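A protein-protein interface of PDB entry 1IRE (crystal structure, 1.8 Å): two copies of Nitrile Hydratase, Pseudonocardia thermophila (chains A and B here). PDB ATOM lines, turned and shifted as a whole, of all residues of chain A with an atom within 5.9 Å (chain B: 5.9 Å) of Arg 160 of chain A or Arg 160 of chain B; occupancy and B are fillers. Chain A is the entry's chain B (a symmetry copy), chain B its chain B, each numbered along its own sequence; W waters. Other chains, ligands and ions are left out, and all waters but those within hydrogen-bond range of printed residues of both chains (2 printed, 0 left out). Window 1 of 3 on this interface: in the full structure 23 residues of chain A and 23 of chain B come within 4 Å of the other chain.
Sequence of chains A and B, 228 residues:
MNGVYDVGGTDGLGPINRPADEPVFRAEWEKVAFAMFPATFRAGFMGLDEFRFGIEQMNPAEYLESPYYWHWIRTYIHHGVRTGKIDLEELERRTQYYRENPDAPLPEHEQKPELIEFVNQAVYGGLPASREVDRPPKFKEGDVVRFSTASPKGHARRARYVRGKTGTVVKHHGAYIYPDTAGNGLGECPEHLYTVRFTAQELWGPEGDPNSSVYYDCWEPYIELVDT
Water W1 lies within hydrogen-bond range of the side-chain amino group (NZ) of Lys 165 of chain B (3.0 Å) and the backbone carbonyl oxygen (O) of Arg 163 of chain A (3.5 Å).
Water W2 lies within hydrogen-bond range of NZ of Lys 165 of chain A (3.0 Å) and O of Arg 163 of chain B (3.5 Å).
Of the 14 printed residues of chain A, 4 touch a printed residue of chain B.
Printed residues of chain A that touch a printed residue of chain B: Asn 2, Val 4, Thr 10 and Arg 160.
Along chain A the printed residues that touch a printed residue of chain B span positions 2 to 160.
Of the 14 printed residues of chain B, 4 touch a printed residue of chain A.
Printed residues of chain B that touch a printed residue of chain A: Asn 2, Val 4, Thr 10 and Arg 160.
Printed residues of chain B within 4 Å of Asn 2 of chain A: Thr 10.
Of the printed residues of chain B, Arg 160 of chain A touches Thr 10 (3.9 Å) and Arg 160 (3.9 Å).
Of the printed residues of chain A, Asn 2 of chain B touches Thr 10 (3.4 Å).
Of the printed residues of chain A, Val 4 of chain B touches Thr 10.
Arg 160 of chain B touches two residues of chain A.
The nearest residue of chain B that does not touch Arg 160 of chain A is Asp 6 of chain B (5.6 Å).
The nearest residue of chain A that does not touch Arg 160 of chain B is Asp 6 of chain A (5.6 Å).
Asn 2 of chain A touches Thr 10 of chain B, and with the chains exchanged Thr 10 of chain A touches Asn 2 of chain B.
Val 4 of chain A touches Thr 10 of chain B, and with the chains exchanged Thr 10 of chain A touches Val 4 of chain B.
Thr 10 of chain A touches Arg 160 of chain B, and with the chains exchanged Arg 160 of chain A touches Thr 10 of chain B.
Arg 160 of chain A touches its own counterpart, Arg 160 of chain B.
Positions printed for both chains: 2, 3, 4, 5, 6, 7, 10, 158, 159, 160, 161, 162, 163 and 165.
O of Val 7 of chain B is in hydrogen-bond range of OG1 of Thr 10 of chain B.
The backbone carbonyl oxygen of Gly 3 of chain B lies within hydrogen-bond range of the guanidinium group of Arg 160 of chain B, at 3.3 Å.
ND2 of Asn 2 of chain B lies close to NH1 of Arg 163 of chain B (2.8 Å).
The guanidinium group (NE) of Arg 160 of chain A lies within salt-bridge range of the side-chain carboxylate (OD2) of Asp 6 of chain A (3.2 Å).
The backbone carbonyl oxygen (O) of Gly 3 of chain A is in hydrogen-bond range of the guanidinium group (NH2) of Arg 160 of chain A (3.3 Å).
OD2 of Asp 6 of chain B lies within salt-bridge range of NE of Arg 160 of chain B (3.2 Å).
Among the printed residues, merely in contact across the chains: Thr 10 of chain A with Asn 2 of chain B (3.4 Å), Asn 2 of chain A with Thr 10 of chain B (3.4 Å), Thr 10 of chain A with Arg 160 of chain B (3.9 Å), Arg 160 of chain A with Thr 10 of chain B (3.9 Å), Arg 160 of chain A with Arg 160 of chain B (3.9 Å), Val 4 of chain A with Thr 10 of chain B (3.97 Å) and Thr 10 of chain A with Val 4 of chain B (3.97 Å).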
ATOM      1  N   ASN A   2      -6.806  23.215  31.660  1.00  0.00           N
ATOM      2  CA  ASN A   2      -7.219  22.522  30.435  1.00  0.00           C
ATOM      3  C   ASN A   2      -6.427  23.119  29.262  1.00  0.00           C
ATOM      4  O   ASN A   2      -7.009  23.626  28.303  1.00  0.00           O
ATOM      5  CB  ASN A   2      -8.718  22.731  30.166  1.00  0.00           C
ATOM      6  CG  ASN A   2      -9.615  22.040  31.177  1.00  0.00           C
ATOM      7  OD1 ASN A   2     -10.829  22.268  31.195  1.00  0.00           O
ATOM      8  ND2 ASN A   2      -9.037  21.185  32.005  1.00  0.00           N
ATOM      9  N   GLY A   3      -5.104  23.051  29.344  1.00  0.00           N
ATOM     10  CA  GLY A   3      -4.273  23.609  28.292  1.00  0.00           C
ATOM     11  C   GLY A   3      -4.106  22.701  27.093  1.00  0.00           C
ATOM     12  O   GLY A   3      -4.273  21.484  27.191  1.00  0.00           O
ATOM     13  N   VAL A   4      -3.786  23.301  25.951  1.00  0.00           N
ATOM     14  CA  VAL A   4      -3.572  22.550  24.720  1.00  0.00           C
ATOM     15  C   VAL A   4      -2.380  21.591  24.862  1.00  0.00           C
ATOM     16  O   VAL A   4      -2.344  20.545  24.210  1.00  0.00           O
ATOM     17  CB  VAL A   4      -3.350  23.503  23.517  1.00  0.00           C
ATOM     18  CG1 VAL A   4      -2.987  22.713  22.269  1.00  0.00           C
ATOM     19  CG2 VAL A   4      -4.613  24.319  23.256  1.00  0.00           C
ATOM     20  N   TYR A   5      -1.430  21.939  25.737  1.00  0.00           N
ATOM     21  CA  TYR A   5      -0.223  21.123  25.989  1.00  0.00           C
ATOM     22  C   TYR A   5      -0.577  19.674  26.370  1.00  0.00           C
ATOM     23  O   TYR A   5       0.224  18.759  26.186  1.00  0.00           O
ATOM     24  CB  TYR A   5       0.610  21.739  27.125  1.00  0.00           C
ATOM     25  CG  TYR A   5       0.088  21.382  28.502  1.00  0.00           C
ATOM     26  CD1 TYR A   5       0.597  20.280  29.194  1.00  0.00           C
ATOM     27  CD2 TYR A   5      -0.981  22.077  29.071  1.00  0.00           C
ATOM     28  CE1 TYR A   5       0.053  19.871  30.402  1.00  0.00           C
ATOM     29  CE2 TYR A   5      -1.534  21.674  30.289  1.00  0.00           C
ATOM     30  CZ  TYR A   5      -1.013  20.570  30.943  1.00  0.00           C
ATOM     31  OH  TYR A   5      -1.571  20.138  32.123  1.00  0.00           O
ATOM     32  N   ASP A   6      -1.748  19.513  26.987  1.00  0.00           N
ATOM     33  CA  ASP A   6      -2.279  18.218  27.430  1.00  0.00           C
ATOM     34  C   ASP A   6      -2.788  17.528  26.152  1.00  0.00           C
ATOM     35  O   ASP A   6      -3.993  17.438  25.906  1.00  0.00           O
ATOM     36  CB  ASP A   6      -3.398  18.522  28.440  1.00  0.00           C
ATOM     37  CG  ASP A   6      -4.201  17.307  28.862  1.00  0.00           C
ATOM     38  OD1 ASP A   6      -3.777  16.157  28.653  1.00  0.00           O
ATOM     39  OD2 ASP A   6      -5.284  17.529  29.434  1.00  0.00           O
ATOM     40  N   VAL A   7      -1.838  17.040  25.354  1.00  0.00           N
ATOM     41  CA  VAL A   7      -2.119  16.432  24.049  1.00  0.00           C
ATOM     42  C   VAL A   7      -2.518  14.961  23.955  1.00  0.00           C
ATOM     43  O   VAL A   7      -2.871  14.501  22.873  1.00  0.00           O
ATOM     44  CB  VAL A   7      -0.942  16.664  23.065  1.00  0.00           C
ATOM     45  CG1 VAL A   7      -0.639  18.150  22.937  1.00  0.00           C
ATOM     46  CG2 VAL A   7       0.301  15.895  23.524  1.00  0.00           C
ATOM     47  N   THR A  10      -5.257  13.778  21.483  1.00  0.00           N
ATOM     48  CA  THR A  10      -5.570  14.793  20.482  1.00  0.00           C
ATOM     49  C   THR A  10      -5.308  14.255  19.072  1.00  0.00           C
ATOM     50  O   THR A  10      -4.302  13.588  18.828  1.00  0.00           O
ATOM     51  CB  THR A  10      -4.745  16.085  20.709  1.00  0.00           C
ATOM     52  OG1 THR A  10      -5.098  16.663  21.970  1.00  0.00           O
ATOM     53  CG2 THR A  10      -5.020  17.109  19.611  1.00  0.00           C
ATOM     54  N   ARG A 158      -3.709  16.184  35.657  1.00  0.00           N
ATOM     55  CA  ARG A 158      -4.986  15.537  35.380  1.00  0.00           C
ATOM     56  C   ARG A 158      -5.285  15.584  33.886  1.00  0.00           C
ATOM     57  O   ARG A 158      -6.116  16.380  33.445  1.00  0.00           O
ATOM     58  CB  ARG A 158      -6.100  16.263  36.141  1.00  0.00           C
ATOM     59  CG  ARG A 158      -5.869  16.373  37.640  1.00  0.00           C
ATOM     60  CD  ARG A 158      -6.785  17.420  38.254  1.00  0.00           C
ATOM     61  NE  ARG A 158      -6.606  17.530  39.700  1.00  0.00           N
ATOM     62  CZ  ARG A 158      -7.420  16.994  40.606  1.00  0.00           C
ATOM     63  NH1 ARG A 158      -8.489  16.299  40.227  1.00  0.00           N
ATOM     64  NH2 ARG A 158      -7.166  17.158  41.899  1.00  0.00           N
ATOM     65  N   ALA A 159      -4.624  14.725  33.112  1.00  0.00           N
ATOM     66  CA  ALA A 159      -4.837  14.692  31.661  1.00  0.00           C
ATOM     67  C   ALA A 159      -6.324  14.550  31.357  1.00  0.00           C
ATOM     68  O   ALA A 159      -7.011  13.714  31.945  1.00  0.00           O
ATOM     69  CB  ALA A 159      -4.059  13.552  31.033  1.00  0.00           C
ATOM     70  N   ARG A 160      -6.825  15.391  30.459  1.00  0.00           N
ATOM     71  CA  ARG A 160      -8.235  15.351  30.113  1.00  0.00           C
ATOM     72  C   ARG A 160      -8.719  13.965  29.695  1.00  0.00           C
ATOM     73  O   ARG A 160      -9.831  13.569  30.050  1.00  0.00           O
ATOM     74  CB  ARG A 160      -8.552  16.377  29.022  1.00  0.00           C
ATOM     75  CG  ARG A 160      -8.606  17.820  29.525  1.00  0.00           C
ATOM     76  CD  ARG A 160      -8.715  18.810  28.362  1.00  0.00           C
ATOM     77  NE  ARG A 160      -7.537  18.738  27.496  1.00  0.00           N
ATOM     78  CZ  ARG A 160      -7.370  19.437  26.376  1.00  0.00           C
ATOM     79  NH1 ARG A 160      -8.308  20.280  25.960  1.00  0.00           N
ATOM     80  NH2 ARG A 160      -6.254  19.293  25.674  1.00  0.00           N
ATOM     81  N   TYR A 161      -7.863  13.194  29.026  1.00  0.00           N
ATOM     82  CA  TYR A 161      -8.270  11.869  28.560  1.00  0.00           C
ATOM     83  C   TYR A 161      -8.578  10.820  29.643  1.00  0.00           C
ATOM     84  O   TYR A 161      -9.252   9.831  29.361  1.00  0.00           O
ATOM     85  CB  TYR A 161      -7.295  11.321  27.500  1.00  0.00           C
ATOM     86  CG  TYR A 161      -6.028  10.672  28.010  1.00  0.00           C
ATOM     87  CD1 TYR A 161      -4.865  11.417  28.212  1.00  0.00           C
ATOM     88  CD2 TYR A 161      -5.977   9.297  28.240  1.00  0.00           C
ATOM     89  CE1 TYR A 161      -3.676  10.801  28.628  1.00  0.00           C
ATOM     90  CE2 TYR A 161      -4.807   8.676  28.652  1.00  0.00           C
ATOM     91  CZ  TYR A 161      -3.661   9.428  28.845  1.00  0.00           C
ATOM     92  OH  TYR A 161      -2.511   8.794  29.247  1.00  0.00           O
ATOM     93  N   VAL A 162      -8.107  11.037  30.870  1.00  0.00           N
ATOM     94  CA  VAL A 162      -8.384  10.078  31.951  1.00  0.00           C
ATOM     95  C   VAL A 162      -9.469  10.534  32.932  1.00  0.00           C
ATOM     96  O   VAL A 162      -9.968   9.731  33.718  1.00  0.00           O
ATOM     97  CB  VAL A 162      -7.116   9.706  32.768  1.00  0.00           C
ATOM     98  CG1 VAL A 162      -6.105   8.999  31.894  1.00  0.00           C
ATOM     99  CG2 VAL A 162      -6.515  10.936  33.430  1.00  0.00           C
ATOM    100  N   ARG A 163      -9.852  11.805  32.872  1.00  0.00           N
ATOM    101  CA  ARG A 163     -10.869  12.329  33.792  1.00  0.00           C
ATOM    102  C   ARG A 163     -12.212  11.609  33.708  1.00  0.00           C
ATOM    103  O   ARG A 163     -12.739  11.366  32.618  1.00  0.00           O
ATOM    104  CB  ARG A 163     -11.073  13.827  33.580  1.00  0.00           C
ATOM    105  CG  ARG A 163      -9.816  14.644  33.810  1.00  0.00           C
ATOM    106  CD  ARG A 163     -10.127  16.125  33.819  1.00  0.00           C
ATOM    107  NE  ARG A 163      -8.913  16.913  33.645  1.00  0.00           N
ATOM    108  CZ  ARG A 163      -8.898  18.204  33.335  1.00  0.00           C
ATOM    109  NH1 ARG A 163     -10.037  18.866  33.180  1.00  0.00           N
ATOM    110  NH2 ARG A 163      -7.743  18.813  33.097  1.00  0.00           N
ATOM    111  N   LYS A 165     -12.787   8.628  34.183  1.00  0.00           N
ATOM    112  CA  LYS A 165     -12.618   7.245  33.755  1.00  0.00           C
ATOM    113  C   LYS A 165     -12.348   6.282  34.909  1.00  0.00           C
ATOM    114  O   LYS A 165     -11.772   6.656  35.932  1.00  0.00           O
ATOM    115  CB  LYS A 165     -11.508   7.139  32.707  1.00  0.00           C
ATOM    116  CG  LYS A 165     -11.768   7.947  31.434  1.00  0.00           C
ATOM    117  CD  LYS A 165     -13.057   7.510  30.749  1.00  0.00           C
ATOM    118  CE  LYS A 165     -13.252   8.193  29.395  1.00  0.00           C
ATOM    119  NZ  LYS A 165     -13.413   9.668  29.499  1.00  0.00           N
ATOM    120  N   ASN B   2     -10.739  14.339  17.747  1.00  0.00           N
ATOM    121  CA  ASN B   2     -10.310  15.048  18.956  1.00  0.00           C
ATOM    122  C   ASN B   2      -9.380  16.194  18.532  1.00  0.00           C
ATOM    123  O   ASN B   2      -8.229  16.263  18.963  1.00  0.00           O
ATOM    124  CB  ASN B   2      -9.531  14.112  19.893  1.00  0.00           C
ATOM    125  CG  ASN B   2     -10.391  13.025  20.513  1.00  0.00           C
ATOM    126  OD1 ASN B   2      -9.869  12.095  21.138  1.00  0.00           O
ATOM    127  ND2 ASN B   2     -11.700  13.138  20.364  1.00  0.00           N
ATOM    128  N   GLY B   3      -9.886  17.089  17.691  1.00  0.00           N
ATOM    129  CA  GLY B   3      -9.074  18.194  17.217  1.00  0.00           C
ATOM    130  C   GLY B   3      -8.990  19.355  18.184  1.00  0.00           C
ATOM    131  O   GLY B   3      -9.856  19.528  19.044  1.00  0.00           O
ATOM    132  N   VAL B   4      -7.934  20.150  18.047  1.00  0.00           N
ATOM    133  CA  VAL B   4      -7.734  21.319  18.895  1.00  0.00           C
ATOM    134  C   VAL B   4      -8.865  22.341  18.695  1.00  0.00           C
ATOM    135  O   VAL B   4      -9.188  23.094  19.616  1.00  0.00           O
ATOM    136  CB  VAL B   4      -6.359  21.981  18.616  1.00  0.00           C
ATOM    137  CG1 VAL B   4      -6.223  23.279  19.399  1.00  0.00           C
ATOM    138  CG2 VAL B   4      -5.232  21.029  19.002  1.00  0.00           C
ATOM    139  N   TYR B   5      -9.475  22.336  17.505  1.00  0.00           N
ATOM    140  CA  TYR B   5     -10.580  23.256  17.159  1.00  0.00           C
ATOM    141  C   TYR B   5     -11.732  23.179  18.176  1.00  0.00           C
ATOM    142  O   TYR B   5     -12.502  24.127  18.331  1.00  0.00           O
ATOM    143  CB  TYR B   5     -11.134  22.922  15.763  1.00  0.00           C
ATOM    144  CG  TYR B   5     -12.110  21.763  15.778  1.00  0.00           C
ATOM    145  CD1 TYR B   5     -13.485  21.989  15.889  1.00  0.00           C
ATOM    146  CD2 TYR B   5     -11.660  20.441  15.782  1.00  0.00           C
ATOM    147  CE1 TYR B   5     -14.381  20.939  16.017  1.00  0.00           C
ATOM    148  CE2 TYR B   5     -12.557  19.377  15.910  1.00  0.00           C
ATOM    149  CZ  TYR B   5     -13.912  19.636  16.031  1.00  0.00           C
ATOM    150  OH  TYR B   5     -14.803  18.602  16.196  1.00  0.00           O
ATOM    151  N   ASP B   6     -11.883  22.004  18.786  1.00  0.00           N
ATOM    152  CA  ASP B   6     -12.913  21.718  19.792  1.00  0.00           C
ATOM    153  C   ASP B   6     -12.418  22.393  21.083  1.00  0.00           C
ATOM    154  O   ASP B   6     -11.953  21.735  22.016  1.00  0.00           O
ATOM    155  CB  ASP B   6     -13.006  20.188  19.906  1.00  0.00           C
ATOM    156  CG  ASP B   6     -13.882  19.703  21.045  1.00  0.00           C
ATOM    157  OD1 ASP B   6     -14.684  20.470  21.604  1.00  0.00           O
ATOM    158  OD2 ASP B   6     -13.762  18.506  21.366  1.00  0.00           O
ATOM    159  N   VAL B   7     -12.538  23.721  21.110  1.00  0.00           N
ATOM    160  CA  VAL B   7     -12.040  24.550  22.213  1.00  0.00           C
ATOM    161  C   VAL B   7     -12.888  24.759  23.465  1.00  0.00           C
ATOM    162  O   VAL B   7     -12.406  25.349  24.428  1.00  0.00           O
ATOM    163  CB  VAL B   7     -11.605  25.949  21.701  1.00  0.00           C
ATOM    164  CG1 VAL B   7     -10.573  25.814  20.591  1.00  0.00           C
ATOM    165  CG2 VAL B   7     -12.821  26.745  21.218  1.00  0.00           C
ATOM    166  N   THR B  10     -11.287  24.790  26.994  1.00  0.00           N
ATOM    167  CA  THR B  10      -9.835  24.928  26.937  1.00  0.00           C
ATOM    168  C   THR B  10      -9.385  26.186  27.688  1.00  0.00           C
ATOM    169  O   THR B  10     -10.005  27.244  27.572  1.00  0.00           O
ATOM    170  CB  THR B  10      -9.328  24.985  25.474  1.00  0.00           C
ATOM    171  OG1 THR B  10      -9.625  23.747  24.817  1.00  0.00           O
ATOM    172  CG2 THR B  10      -7.819  25.209  25.426  1.00  0.00           C
ATOM    173  N   ARG B 158     -19.193  15.949  18.722  1.00  0.00           N
ATOM    174  CA  ARG B 158     -19.075  15.422  20.076  1.00  0.00           C
ATOM    175  C   ARG B 158     -17.990  16.171  20.840  1.00  0.00           C
ATOM    176  O   ARG B 158     -16.893  15.644  21.033  1.00  0.00           O
ATOM    177  CB  ARG B 158     -18.714  13.934  20.014  1.00  0.00           C
ATOM    178  CG  ARG B 158     -19.673  13.088  19.190  1.00  0.00           C
ATOM    179  CD  ARG B 158     -19.052  11.742  18.850  1.00  0.00           C
ATOM    180  NE  ARG B 158     -19.960  10.895  18.081  1.00  0.00           N
ATOM    181  CZ  ARG B 158     -20.669   9.889  18.589  1.00  0.00           C
ATOM    182  NH1 ARG B 158     -20.584   9.588  19.881  1.00  0.00           N
ATOM    183  NH2 ARG B 158     -21.464   9.178  17.798  1.00  0.00           N
ATOM    184  N   ALA B 159     -18.298  17.388  21.285  1.00  0.00           N
ATOM    185  CA  ALA B 159     -17.322  18.193  22.029  1.00  0.00           C
ATOM    186  C   ALA B 159     -16.770  17.389  23.200  1.00  0.00           C
ATOM    187  O   ALA B 159     -17.523  16.767  23.949  1.00  0.00           O
ATOM    188  CB  ALA B 159     -17.957  19.479  22.523  1.00  0.00           C
ATOM    189  N   ARG B 160     -15.449  17.378  23.336  1.00  0.00           N
ATOM    190  CA  ARG B 160     -14.821  16.626  24.410  1.00  0.00           C
ATOM    191  C   ARG B 160     -15.376  16.961  25.792  1.00  0.00           C
ATOM    192  O   ARG B 160     -15.540  16.065  26.621  1.00  0.00           O
ATOM    193  CB  ARG B 160     -13.302  16.816  24.384  1.00  0.00           C
ATOM    194  CG  ARG B 160     -12.597  16.033  23.277  1.00  0.00           C
ATOM    195  CD  ARG B 160     -11.121  16.427  23.171  1.00  0.00           C
ATOM    196  NE  ARG B 160     -10.976  17.837  22.809  1.00  0.00           N
ATOM    197  CZ  ARG B 160      -9.817  18.481  22.697  1.00  0.00           C
ATOM    198  NH1 ARG B 160      -8.669  17.848  22.920  1.00  0.00           N
ATOM    199  NH2 ARG B 160      -9.808  19.762  22.356  1.00  0.00           N
ATOM    200  N   TYR B 161     -15.749  18.220  26.012  1.00  0.00           N
ATOM    201  CA  TYR B 161     -16.253  18.623  27.324  1.00  0.00           C
ATOM    202  C   TYR B 161     -17.590  18.006  27.769  1.00  0.00           C
ATOM    203  O   TYR B 161     -17.897  18.004  28.961  1.00  0.00           O
ATOM    204  CB  TYR B 161     -16.254  20.156  27.480  1.00  0.00           C
ATOM    205  CG  TYR B 161     -17.427  20.901  26.883  1.00  0.00           C
ATOM    206  CD1 TYR B 161     -17.392  21.370  25.568  1.00  0.00           C
ATOM    207  CD2 TYR B 161     -18.555  21.186  27.653  1.00  0.00           C
ATOM    208  CE1 TYR B 161     -18.456  22.111  25.037  1.00  0.00           C
ATOM    209  CE2 TYR B 161     -19.615  21.918  27.138  1.00  0.00           C
ATOM    210  CZ  TYR B 161     -19.563  22.378  25.834  1.00  0.00           C
ATOM    211  OH  TYR B 161     -20.620  23.108  25.345  1.00  0.00           O
ATOM    212  N   VAL B 162     -18.373  17.475  26.831  1.00  0.00           N
ATOM    213  CA  VAL B 162     -19.656  16.856  27.197  1.00  0.00           C
ATOM    214  C   VAL B 162     -19.634  15.323  27.204  1.00  0.00           C
ATOM    215  O   VAL B 162     -20.550  14.694  27.732  1.00  0.00           O
ATOM    216  CB  VAL B 162     -20.831  17.320  26.295  1.00  0.00           C
ATOM    217  CG1 VAL B 162     -21.076  18.804  26.457  1.00  0.00           C
ATOM    218  CG2 VAL B 162     -20.579  16.954  24.841  1.00  0.00           C
ATOM    219  N   ARG B 163     -18.586  14.725  26.647  1.00  0.00           N
ATOM    220  CA  ARG B 163     -18.498  13.260  26.589  1.00  0.00           C
ATOM    221  C   ARG B 163     -18.537  12.582  27.956  1.00  0.00           C
ATOM    222  O   ARG B 163     -17.845  12.993  28.892  1.00  0.00           O
ATOM    223  CB  ARG B 163     -17.249  12.821  25.830  1.00  0.00           C
ATOM    224  CG  ARG B 163     -17.209  13.315  24.397  1.00  0.00           C
ATOM    225  CD  ARG B 163     -16.081  12.662  23.630  1.00  0.00           C
ATOM    226  NE  ARG B 163     -15.789  13.398  22.405  1.00  0.00           N
ATOM    227  CZ  ARG B 163     -14.689  13.236  21.680  1.00  0.00           C
ATOM    228  NH1 ARG B 163     -13.776  12.346  22.044  1.00  0.00           N
ATOM    229  NH2 ARG B 163     -14.463  14.023  20.637  1.00  0.00           N
ATOM    230  N   LYS B 165     -20.757  12.735  30.075  1.00  0.00           N
ATOM    231  CA  LYS B 165     -21.503  13.532  31.039  1.00  0.00           C
ATOM    232  C   LYS B 165     -23.004  13.250  31.027  1.00  0.00           C
ATOM    233  O   LYS B 165     -23.577  12.881  30.002  1.00  0.00           O
ATOM    234  CB  LYS B 165     -21.244  15.024  30.816  1.00  0.00           C
ATOM    235  CG  LYS B 165     -19.779  15.437  30.970  1.00  0.00           C
ATOM    236  CD  LYS B 165     -19.249  15.105  32.360  1.00  0.00           C
ATOM    237  CE  LYS B 165     -17.839  15.652  32.586  1.00  0.00           C
ATOM    238  NZ  LYS B 165     -16.821  15.044  31.687  1.00  0.00           N
HETATM  239  O   HOH W   1     -13.994  14.150  30.978  1.00  0.00           O
HETATM  240  O   HOH W   2     -14.450  12.373  28.547  1.00  0.00           O
